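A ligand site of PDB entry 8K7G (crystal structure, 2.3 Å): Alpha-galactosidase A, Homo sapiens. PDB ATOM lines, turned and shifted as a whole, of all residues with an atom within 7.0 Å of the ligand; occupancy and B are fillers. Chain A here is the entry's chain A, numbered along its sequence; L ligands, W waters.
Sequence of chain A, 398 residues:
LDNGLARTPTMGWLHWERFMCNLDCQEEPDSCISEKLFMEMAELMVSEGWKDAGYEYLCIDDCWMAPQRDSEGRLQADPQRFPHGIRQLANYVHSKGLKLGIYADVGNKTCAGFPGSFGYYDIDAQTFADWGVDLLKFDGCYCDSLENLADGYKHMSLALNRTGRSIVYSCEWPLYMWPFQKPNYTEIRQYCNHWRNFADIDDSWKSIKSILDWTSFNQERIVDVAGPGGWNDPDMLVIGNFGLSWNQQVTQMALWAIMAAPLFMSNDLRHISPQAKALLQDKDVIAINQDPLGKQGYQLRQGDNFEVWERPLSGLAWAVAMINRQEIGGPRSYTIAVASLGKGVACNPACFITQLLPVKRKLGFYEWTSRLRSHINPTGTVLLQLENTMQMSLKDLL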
ATOM      1  N   LEU A  14     -28.981  17.102  -0.780  1.00  0.00           N
ATOM      2  CA  LEU A  14     -27.956  17.429  -1.770  1.00  0.00           C
ATOM      3  C   LEU A  14     -28.651  17.889  -3.054  1.00  0.00           C
ATOM      4  O   LEU A  14     -29.594  17.229  -3.509  1.00  0.00           O
ATOM      5  CB  LEU A  14     -27.076  16.221  -2.030  1.00  0.00           C
ATOM      6  CG  LEU A  14     -25.897  16.290  -2.978  1.00  0.00           C
ATOM      7  CD1 LEU A  14     -24.874  17.309  -2.487  1.00  0.00           C
ATOM      8  CD2 LEU A  14     -25.279  14.903  -3.044  1.00  0.00           C
ATOM      9  N   TRP A  16     -27.839  18.044  -6.295  1.00  0.00           N
ATOM     10  CA  TRP A  16     -27.424  17.722  -7.667  1.00  0.00           C
ATOM     11  C   TRP A  16     -28.555  17.149  -8.520  1.00  0.00           C
ATOM     12  O   TRP A  16     -28.790  17.640  -9.636  1.00  0.00           O
ATOM     13  CB  TRP A  16     -26.242  16.773  -7.708  1.00  0.00           C
ATOM     14  CG  TRP A  16     -25.825  16.611  -9.126  1.00  0.00           C
ATOM     15  CD1 TRP A  16     -25.993  15.518  -9.924  1.00  0.00           C
ATOM     16  CD2 TRP A  16     -25.221  17.618  -9.959  1.00  0.00           C
ATOM     17  NE1 TRP A  16     -25.493  15.771 -11.191  1.00  0.00           N
ATOM     18  CE2 TRP A  16     -25.029  17.056 -11.235  1.00  0.00           C
ATOM     19  CE3 TRP A  16     -24.828  18.948  -9.746  1.00  0.00           C
ATOM     20  CZ2 TRP A  16     -24.457  17.771 -12.292  1.00  0.00           C
ATOM     21  CZ3 TRP A  16     -24.266  19.659 -10.795  1.00  0.00           C
ATOM     22  CH2 TRP A  16     -24.074  19.060 -12.051  1.00  0.00           C
ATOM     23  N   CYS A  21     -26.765  21.904 -12.609  1.00  0.00           N
ATOM     24  CA  CYS A  21     -25.873  23.043 -12.721  1.00  0.00           C
ATOM     25  C   CYS A  21     -26.585  24.239 -13.325  1.00  0.00           C
ATOM     26  O   CYS A  21     -26.109  24.830 -14.296  1.00  0.00           O
ATOM     27  CB  CYS A  21     -24.646  22.674 -13.570  1.00  0.00           C
ATOM     28  SG  CYS A  21     -23.297  23.848 -13.479  1.00  0.00           S
ATOM     29  N   ASP A  61     -23.602  20.855  -4.008  1.00  0.00           N
ATOM     30  CA  ASP A  61     -22.885  20.040  -4.974  1.00  0.00           C
ATOM     31  C   ASP A  61     -22.137  20.953  -5.937  1.00  0.00           C
ATOM     32  O   ASP A  61     -21.808  22.087  -5.580  1.00  0.00           O
ATOM     33  CB  ASP A  61     -23.848  19.088  -5.711  1.00  0.00           C
ATOM     34  CG  ASP A  61     -23.168  17.783  -6.173  1.00  0.00           C
ATOM     35  OD1 ASP A  61     -22.512  17.811  -7.219  1.00  0.00           O
ATOM     36  OD2 ASP A  61     -23.290  16.746  -5.503  1.00  0.00           O
ATOM     37  N   ASP A  62     -21.871  20.476  -7.148  1.00  0.00           N
ATOM     38  CA  ASP A  62     -21.077  21.239  -8.105  1.00  0.00           C
ATOM     39  C   ASP A  62     -21.788  22.521  -8.508  1.00  0.00           C
ATOM     40  O   ASP A  62     -23.011  22.658  -8.375  1.00  0.00           O
ATOM     41  CB  ASP A  62     -20.790  20.390  -9.348  1.00  0.00           C
ATOM     42  CG  ASP A  62     -19.563  20.850 -10.128  1.00  0.00           C
ATOM     43  OD1 ASP A  62     -19.027  21.946  -9.829  1.00  0.00           O
ATOM     44  OD2 ASP A  62     -19.145  20.118 -11.041  1.00  0.00           O
ATOM     45  N   CYS A  63     -20.989  23.484  -8.998  1.00  0.00           N
ATOM     46  CA  CYS A  63     -21.428  24.760  -9.578  1.00  0.00           C
ATOM     47  C   CYS A  63     -21.765  25.816  -8.531  1.00  0.00           C
ATOM     48  O   CYS A  63     -22.648  26.645  -8.757  1.00  0.00           O
ATOM     49  CB  CYS A  63     -22.608  24.575 -10.530  1.00  0.00           C
ATOM     50  SG  CYS A  63     -22.285  23.303 -11.780  1.00  0.00           S
ATOM     51  N   TYR A 103     -18.693  20.875  -2.069  1.00  0.00           N
ATOM     52  CA  TYR A 103     -18.221  19.992  -3.125  1.00  0.00           C
ATOM     53  C   TYR A 103     -16.863  20.478  -3.655  1.00  0.00           C
ATOM     54  O   TYR A 103     -16.609  21.685  -3.737  1.00  0.00           O
ATOM     55  CB  TYR A 103     -19.263  19.943  -4.273  1.00  0.00           C
ATOM     56  CG  TYR A 103     -18.792  19.339  -5.586  1.00  0.00           C
ATOM     57  CD1 TYR A 103     -18.040  20.087  -6.482  1.00  0.00           C
ATOM     58  CD2 TYR A 103     -19.153  18.052  -5.957  1.00  0.00           C
ATOM     59  CE1 TYR A 103     -17.618  19.553  -7.682  1.00  0.00           C
ATOM     60  CE2 TYR A 103     -18.750  17.507  -7.162  1.00  0.00           C
ATOM     61  CZ  TYR A 103     -17.970  18.261  -8.018  1.00  0.00           C
ATOM     62  OH  TYR A 103     -17.553  17.743  -9.217  1.00  0.00           O
ATOM     63  N   ASP A 105     -13.250  18.748  -6.283  1.00  0.00           N
ATOM     64  CA  ASP A 105     -12.820  17.714  -7.218  1.00  0.00           C
ATOM     65  C   ASP A 105     -11.328  17.447  -7.047  1.00  0.00           C
ATOM     66  O   ASP A 105     -10.538  18.377  -6.862  1.00  0.00           O
ATOM     67  CB  ASP A 105     -13.157  18.114  -8.675  1.00  0.00           C
ATOM     68  CG  ASP A 105     -13.035  16.936  -9.661  1.00  0.00           C
ATOM     69  OD1 ASP A 105     -11.898  16.480  -9.921  1.00  0.00           O
ATOM     70  OD2 ASP A 105     -14.077  16.454 -10.143  1.00  0.00           O
ATOM     71  N   THR A 110     -13.542  20.632 -11.782  1.00  0.00           N
ATOM     72  CA  THR A 110     -14.713  19.866 -11.384  1.00  0.00           C
ATOM     73  C   THR A 110     -15.372  19.272 -12.619  1.00  0.00           C
ATOM     74  O   THR A 110     -15.012  19.603 -13.756  1.00  0.00           O
ATOM     75  CB  THR A 110     -15.720  20.732 -10.616  1.00  0.00           C
ATOM     76  OG1 THR A 110     -16.366  21.644 -11.517  1.00  0.00           O
ATOM     77  CG2 THR A 110     -15.045  21.498  -9.478  1.00  0.00           C
ATOM     78  N   CYS A 111     -16.319  18.359 -12.418  1.00  0.00           N
ATOM     79  CA  CYS A 111     -16.989  17.752 -13.574  1.00  0.00           C
ATOM     80  C   CYS A 111     -17.693  18.801 -14.431  1.00  0.00           C
ATOM     81  O   CYS A 111     -17.779  18.624 -15.649  1.00  0.00           O
ATOM     82  CB  CYS A 111     -17.961  16.656 -13.133  1.00  0.00           C
ATOM     83  SG  CYS A 111     -17.148  15.184 -12.432  1.00  0.00           S
ATOM     84  N   ALA A 112     -18.155  19.893 -13.832  1.00  0.00           N
ATOM     85  CA  ALA A 112     -18.814  20.950 -14.587  1.00  0.00           C
ATOM     86  C   ALA A 112     -17.845  21.991 -15.157  1.00  0.00           C
ATOM     87  O   ALA A 112     -18.280  22.873 -15.910  1.00  0.00           O
ATOM     88  CB  ALA A 112     -19.858  21.648 -13.698  1.00  0.00           C
ATOM     89  N   GLY A 113     -16.562  21.909 -14.840  1.00  0.00           N
ATOM     90  CA  GLY A 113     -15.564  22.773 -15.438  1.00  0.00           C
ATOM     91  C   GLY A 113     -15.068  23.906 -14.572  1.00  0.00           C
ATOM     92  O   GLY A 113     -14.409  24.823 -15.099  1.00  0.00           O
ATOM     93  N   LYS A 137     -17.897  16.514  -0.341  1.00  0.00           N
ATOM     94  CA  LYS A 137     -18.049  15.557  -1.436  1.00  0.00           C
ATOM     95  C   LYS A 137     -16.953  15.852  -2.456  1.00  0.00           C
ATOM     96  O   LYS A 137     -16.829  16.999  -2.924  1.00  0.00           O
ATOM     97  CB  LYS A 137     -19.438  15.667  -2.069  1.00  0.00           C
ATOM     98  CG  LYS A 137     -19.790  14.554  -3.062  1.00  0.00           C
ATOM     99  CD  LYS A 137     -20.815  15.006  -4.108  1.00  0.00           C
ATOM    100  CE  LYS A 137     -21.133  13.904  -5.112  1.00  0.00           C
ATOM    101  NZ  LYS A 137     -22.289  14.212  -6.005  1.00  0.00           N
ATOM    102  N   ASP A 139     -15.164  14.867  -5.893  1.00  0.00           N
ATOM    103  CA  ASP A 139     -15.418  14.233  -7.176  1.00  0.00           C
ATOM    104  C   ASP A 139     -14.099  13.853  -7.858  1.00  0.00           C
ATOM    105  O   ASP A 139     -13.022  14.315  -7.485  1.00  0.00           O
ATOM    106  CB  ASP A 139     -16.237  15.206  -8.038  1.00  0.00           C
ATOM    107  CG  ASP A 139     -17.160  14.502  -9.014  1.00  0.00           C
ATOM    108  OD1 ASP A 139     -16.990  13.289  -9.288  1.00  0.00           O
ATOM    109  OD2 ASP A 139     -18.093  15.179  -9.487  1.00  0.00           O
ATOM    110  N   GLY A 140     -14.192  13.006  -8.885  1.00  0.00           N
ATOM    111  CA  GLY A 140     -12.993  12.492  -9.544  1.00  0.00           C
ATOM    112  C   GLY A 140     -12.772  12.824 -11.015  1.00  0.00           C
ATOM    113  O   GLY A 140     -12.013  12.120 -11.677  1.00  0.00           O
ATOM    114  N   CYS A 141     -13.389  13.899 -11.532  1.00  0.00           N
ATOM    115  CA  CYS A 141     -13.212  14.256 -12.941  1.00  0.00           C
ATOM    116  C   CYS A 141     -11.852  14.908 -13.183  1.00  0.00           C
ATOM    117  O   CYS A 141     -11.205  15.418 -12.262  1.00  0.00           O
ATOM    118  CB  CYS A 141     -14.299  15.231 -13.413  1.00  0.00           C
ATOM    119  SG  CYS A 141     -15.871  14.501 -13.899  1.00  0.00           S
ATOM    120  N   GLU A 172     -15.605   9.789  -4.278  1.00  0.00           N
ATOM    121  CA  GLU A 172     -16.035   9.068  -5.482  1.00  0.00           C
ATOM    122  C   GLU A 172     -14.915   8.214  -6.056  1.00  0.00           C
ATOM    123  O   GLU A 172     -15.006   7.729  -7.188  1.00  0.00           O
ATOM    124  CB  GLU A 172     -16.577  10.044  -6.535  1.00  0.00           C
ATOM    125  CG  GLU A 172     -17.822  10.809  -6.107  1.00  0.00           C
ATOM    126  CD  GLU A 172     -18.685  11.267  -7.275  1.00  0.00           C
ATOM    127  OE1 GLU A 172     -18.884  10.469  -8.227  1.00  0.00           O
ATOM    128  OE2 GLU A 172     -19.139  12.422  -7.266  1.00  0.00           O
ATOM    129  N   LEU A 175     -15.725   4.699  -7.850  1.00  0.00           N
ATOM    130  CA  LEU A 175     -16.408   4.896  -9.127  1.00  0.00           C
ATOM    131  C   LEU A 175     -15.419   5.231 -10.249  1.00  0.00           C
ATOM    132  O   LEU A 175     -15.523   4.681 -11.354  1.00  0.00           O
ATOM    133  CB  LEU A 175     -17.444   6.029  -8.989  1.00  0.00           C
ATOM    134  CG  LEU A 175     -18.127   6.480 -10.275  1.00  0.00           C
ATOM    135  CD1 LEU A 175     -18.863   5.294 -10.898  1.00  0.00           C
ATOM    136  CD2 LEU A 175     -19.097   7.656 -10.029  1.00  0.00           C
ATOM    137  N   TYR A 176     -14.438   6.093  -9.971  1.00  0.00           N
ATOM    138  CA  TYR A 176     -13.486   6.449 -11.011  1.00  0.00           C
ATOM    139  C   TYR A 176     -12.366   5.427 -11.169  1.00  0.00           C
ATOM    140  O   TYR A 176     -11.700   5.409 -12.210  1.00  0.00           O
ATOM    141  CB  TYR A 176     -12.903   7.837 -10.737  1.00  0.00           C
ATOM    142  CG  TYR A 176     -13.924   8.915 -10.950  1.00  0.00           C
ATOM    143  CD1 TYR A 176     -14.086   9.506 -12.193  1.00  0.00           C
ATOM    144  CD2 TYR A 176     -14.751   9.337  -9.905  1.00  0.00           C
ATOM    145  CE1 TYR A 176     -15.046  10.499 -12.400  1.00  0.00           C
ATOM    146  CE2 TYR A 176     -15.723  10.326 -10.104  1.00  0.00           C
ATOM    147  CZ  TYR A 176     -15.857  10.908 -11.363  1.00  0.00           C
ATOM    148  OH  TYR A 176     -16.802  11.888 -11.579  1.00  0.00           O
ATOM    149  N   ARG A 196     -18.867   6.585  -3.296  1.00  0.00           N
ATOM    150  CA  ARG A 196     -19.708   6.265  -4.442  1.00  0.00           C
ATOM    151  C   ARG A 196     -19.111   5.097  -5.226  1.00  0.00           C
ATOM    152  O   ARG A 196     -17.936   5.111  -5.614  1.00  0.00           O
ATOM    153  CB  ARG A 196     -19.838   7.498  -5.338  1.00  0.00           C
ATOM    154  CG  ARG A 196     -20.826   8.540  -4.808  1.00  0.00           C
ATOM    155  CD  ARG A 196     -22.265   8.132  -5.165  1.00  0.00           C
ATOM    156  NE  ARG A 196     -22.382   7.829  -6.582  1.00  0.00           N
ATOM    157  CZ  ARG A 196     -22.413   8.740  -7.552  1.00  0.00           C
ATOM    158  NH1 ARG A 196     -22.426  10.048  -7.271  1.00  0.00           N
ATOM    159  NH2 ARG A 196     -22.416   8.343  -8.819  1.00  0.00           N
ATOM    160  N   PHE A 198     -21.026   3.455  -8.031  1.00  0.00           N
ATOM    161  CA  PHE A 198     -21.669   3.176  -9.309  1.00  0.00           C
ATOM    162  C   PHE A 198     -22.122   4.499  -9.936  1.00  0.00           C
ATOM    163  O   PHE A 198     -22.088   5.548  -9.303  1.00  0.00           O
ATOM    164  CB  PHE A 198     -22.835   2.193  -9.116  1.00  0.00           C
ATOM    165  CG  PHE A 198     -23.515   1.777 -10.409  1.00  0.00           C
ATOM    166  CD1 PHE A 198     -22.841   0.996 -11.355  1.00  0.00           C
ATOM    167  CD2 PHE A 198     -24.826   2.163 -10.688  1.00  0.00           C
ATOM    168  CE1 PHE A 198     -23.449   0.620 -12.533  1.00  0.00           C
ATOM    169  CE2 PHE A 198     -25.445   1.782 -11.857  1.00  0.00           C
ATOM    170  CZ  PHE A 198     -24.757   1.005 -12.784  1.00  0.00           C
ATOM    171  N   ALA A 199     -22.556   4.413 -11.203  1.00  0.00           N
ATOM    172  CA  ALA A 199     -22.923   5.583 -11.991  1.00  0.00           C
ATOM    173  C   ALA A 199     -24.004   6.426 -11.308  1.00  0.00           C
ATOM    174  O   ALA A 199     -24.826   5.929 -10.527  1.00  0.00           O
ATOM    175  CB  ALA A 199     -23.420   5.160 -13.373  1.00  0.00           C
ATOM    176  N   ASP A 200     -24.011   7.721 -11.653  1.00  0.00           N
ATOM    177  CA  ASP A 200     -24.958   8.681 -11.080  1.00  0.00           C
ATOM    178  C   ASP A 200     -26.401   8.200 -11.217  1.00  0.00           C
ATOM    179  O   ASP A 200     -26.811   7.688 -12.262  1.00  0.00           O
ATOM    180  CB  ASP A 200     -24.825  10.037 -11.786  1.00  0.00           C
ATOM    181  CG  ASP A 200     -23.465  10.676 -11.566  1.00  0.00           C
ATOM    182  OD1 ASP A 200     -22.653  10.150 -10.757  1.00  0.00           O
ATOM    183  OD2 ASP A 200     -23.217  11.730 -12.205  1.00  0.00           O
ATOM    184  N   ILE A 201     -27.173   8.403 -10.161  1.00  0.00           N
ATOM    185  CA  ILE A 201     -28.608   8.149 -10.208  1.00  0.00           C
ATOM    186  C   ILE A 201     -29.291   9.233 -11.045  1.00  0.00           C
ATOM    187  O   ILE A 201     -28.820  10.384 -11.129  1.00  0.00           O
ATOM    188  CB  ILE A 201     -29.187   8.106  -8.794  1.00  0.00           C
ATOM    189  CG1 ILE A 201     -30.593   7.502  -8.788  1.00  0.00           C
ATOM    190  CG2 ILE A 201     -29.244   9.516  -8.193  1.00  0.00           C
ATOM    191  CD1 ILE A 201     -30.990   6.932  -7.454  1.00  0.00           C
ATOM    192  N   ASP A 235     -25.773   6.487  -4.028  1.00  0.00           N
ATOM    193  CA  ASP A 235     -26.214   7.795  -4.535  1.00  0.00           C
ATOM    194  C   ASP A 235     -27.577   8.204  -3.962  1.00  0.00           C
ATOM    195  O   ASP A 235     -28.153   7.493  -3.118  1.00  0.00           O
ATOM    196  CB  ASP A 235     -26.216   7.840  -6.069  1.00  0.00           C
ATOM    197  CG  ASP A 235     -25.845   9.222  -6.614  1.00  0.00           C
ATOM    198  OD1 ASP A 235     -25.607  10.147  -5.798  1.00  0.00           O
ATOM    199  OD2 ASP A 235     -25.802   9.386  -7.872  1.00  0.00           O
ATOM    200  N   MET A 236     -28.081   9.346  -4.432  1.00  0.00           N
ATOM    201  CA  MET A 236     -29.125  10.096  -3.741  1.00  0.00           C
ATOM    202  C   MET A 236     -30.504   9.431  -3.789  1.00  0.00           C
ATOM    203  O   MET A 236     -30.838   8.688  -4.726  1.00  0.00           O
ATOM    204  CB  MET A 236     -29.240  11.500  -4.342  1.00  0.00           C
ATOM    205  CG  MET A 236     -27.902  12.255  -4.394  1.00  0.00           C
ATOM    206  SD  MET A 236     -27.987  13.723  -5.467  1.00  0.00           S
ATOM    207  CE  MET A 236     -27.283  13.041  -6.968  1.00  0.00           C
HETATM  208  C1  LIG L   1     -21.566  15.734 -10.604  1.00  0.00           C
HETATM  209  C2  LIG L   1     -22.345  15.199  -9.437  1.00  0.00           C
HETATM  210  C3  LIG L   1     -21.117  17.166 -10.295  1.00  0.00           C
HETATM  211  C4  LIG L   1     -22.236  13.715  -9.718  1.00  0.00           C
HETATM  212  C5  LIG L   1     -20.716  13.610  -9.916  1.00  0.00           C
HETATM  213  C6  LIG L   1     -20.287  12.403 -10.784  1.00  0.00           C
HETATM  214  N1  LIG L   1     -20.390  14.838 -10.666  1.00  0.00           N
HETATM  215  O1  LIG L   1     -21.641  15.554  -8.213  1.00  0.00           O
HETATM  216  O2  LIG L   1     -22.672  12.988  -8.569  1.00  0.00           O
HETATM  217  O3  LIG L   1     -20.377  17.734 -11.401  1.00  0.00           O
HETATM  218  O4  LIG L   1     -20.530  11.156 -10.128  1.00  0.00           O
HETATM  219  O   HOH W   1     -25.015  11.701  -8.664  1.00  0.00           O
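Trp 16 touches the ligand (NE1 to C2, 3.6 Å). Tyr 103 touches the ligand (OH to O3, 3.6 Å). Ala 112 touches the ligand (N to O3, 3.9 Å). CD2 of Leu 175 touches O4 of the ligand (3.8 Å). OH of Tyr 176 touches C6 of the ligand (3.6 Å). Hydrophobic or aromatic side chains that line the ligand: Trp 16, Tyr 103 and Leu 175. 13 residues have an atom within 4 Å of the ligand: Trp 16, Asp 61, Asp 62, Tyr 103, Cys 111, Ala 112, Lys 137, Asp 139, Glu 172, Leu 175, Tyr 176, Arg 196 and Asp 200. The nearest printed residue that does not touch the ligand is Asp 235 (4.8 Å).
Water W1 lies within hydrogen-bond range of the side-chain carboxylate (OD2) of Asp 235 (2.6 Å), an oxygen (O2) of the ligand (2.7 Å) and the guanidinium group (NH1) of Arg 196 (3.4 Å).
OH of Tyr 176 is in hydrogen-bond range of OD1 of Asp 139 (2.7 Å). The guanidinium group (NH1) of Arg 196 is in salt-bridge range of the side-chain carboxylate (OE1) of Glu 172 (3.7 Å). NZ of Lys 137 is in salt-bridge range of OD2 of Asp 61 (2.8 Å). OD2 of Asp 62 is in hydrogen-bond range of OH of Tyr 103 (3.4 Å). OD2 of Asp 62 sits at hydrogen-bond distance from N of Ala 112, at 3.0 Å. The backbone NH (N) of Cys 111 sits at hydrogen-bond distance from the side-chain hydroxyl (OH) of Tyr 103 (3.5 Å). O of Arg 196 is in hydrogen-bond range of N of Leu 175. SG of Cys 63 is disulfide-bonded to SG of Cys 21, 2.1 Å away.
The side-chain carboxylate (OD1) of Asp 200 is in hydrogen-bond range of an oxygen (O4) of the ligand. A nitrogen (N1) of the ligand is in salt-bridge range of the side-chain carboxylate (OD2) of Asp 139 (2.6 Å). OE1 of Glu 172 lies within hydrogen-bond range of O4 of the ligand, at 2.6 Å. O1 of the ligand is in hydrogen-bond range of OD1 of Asp 61, 2.6 Å away. NZ of Lys 137 is in hydrogen-bond range of O1 of the ligand, 2.7 Å away. The side-chain carboxylate (OD2) of Asp 62 lies within hydrogen-bond range of an oxygen (O3) of the ligand, 2.7 Å away. SG of Cys 111 is in hydrogen-bond range of N1 of the ligand, at 3.7 Å. NH1 of Arg 196 sits at hydrogen-bond distance from O2 of the ligand.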
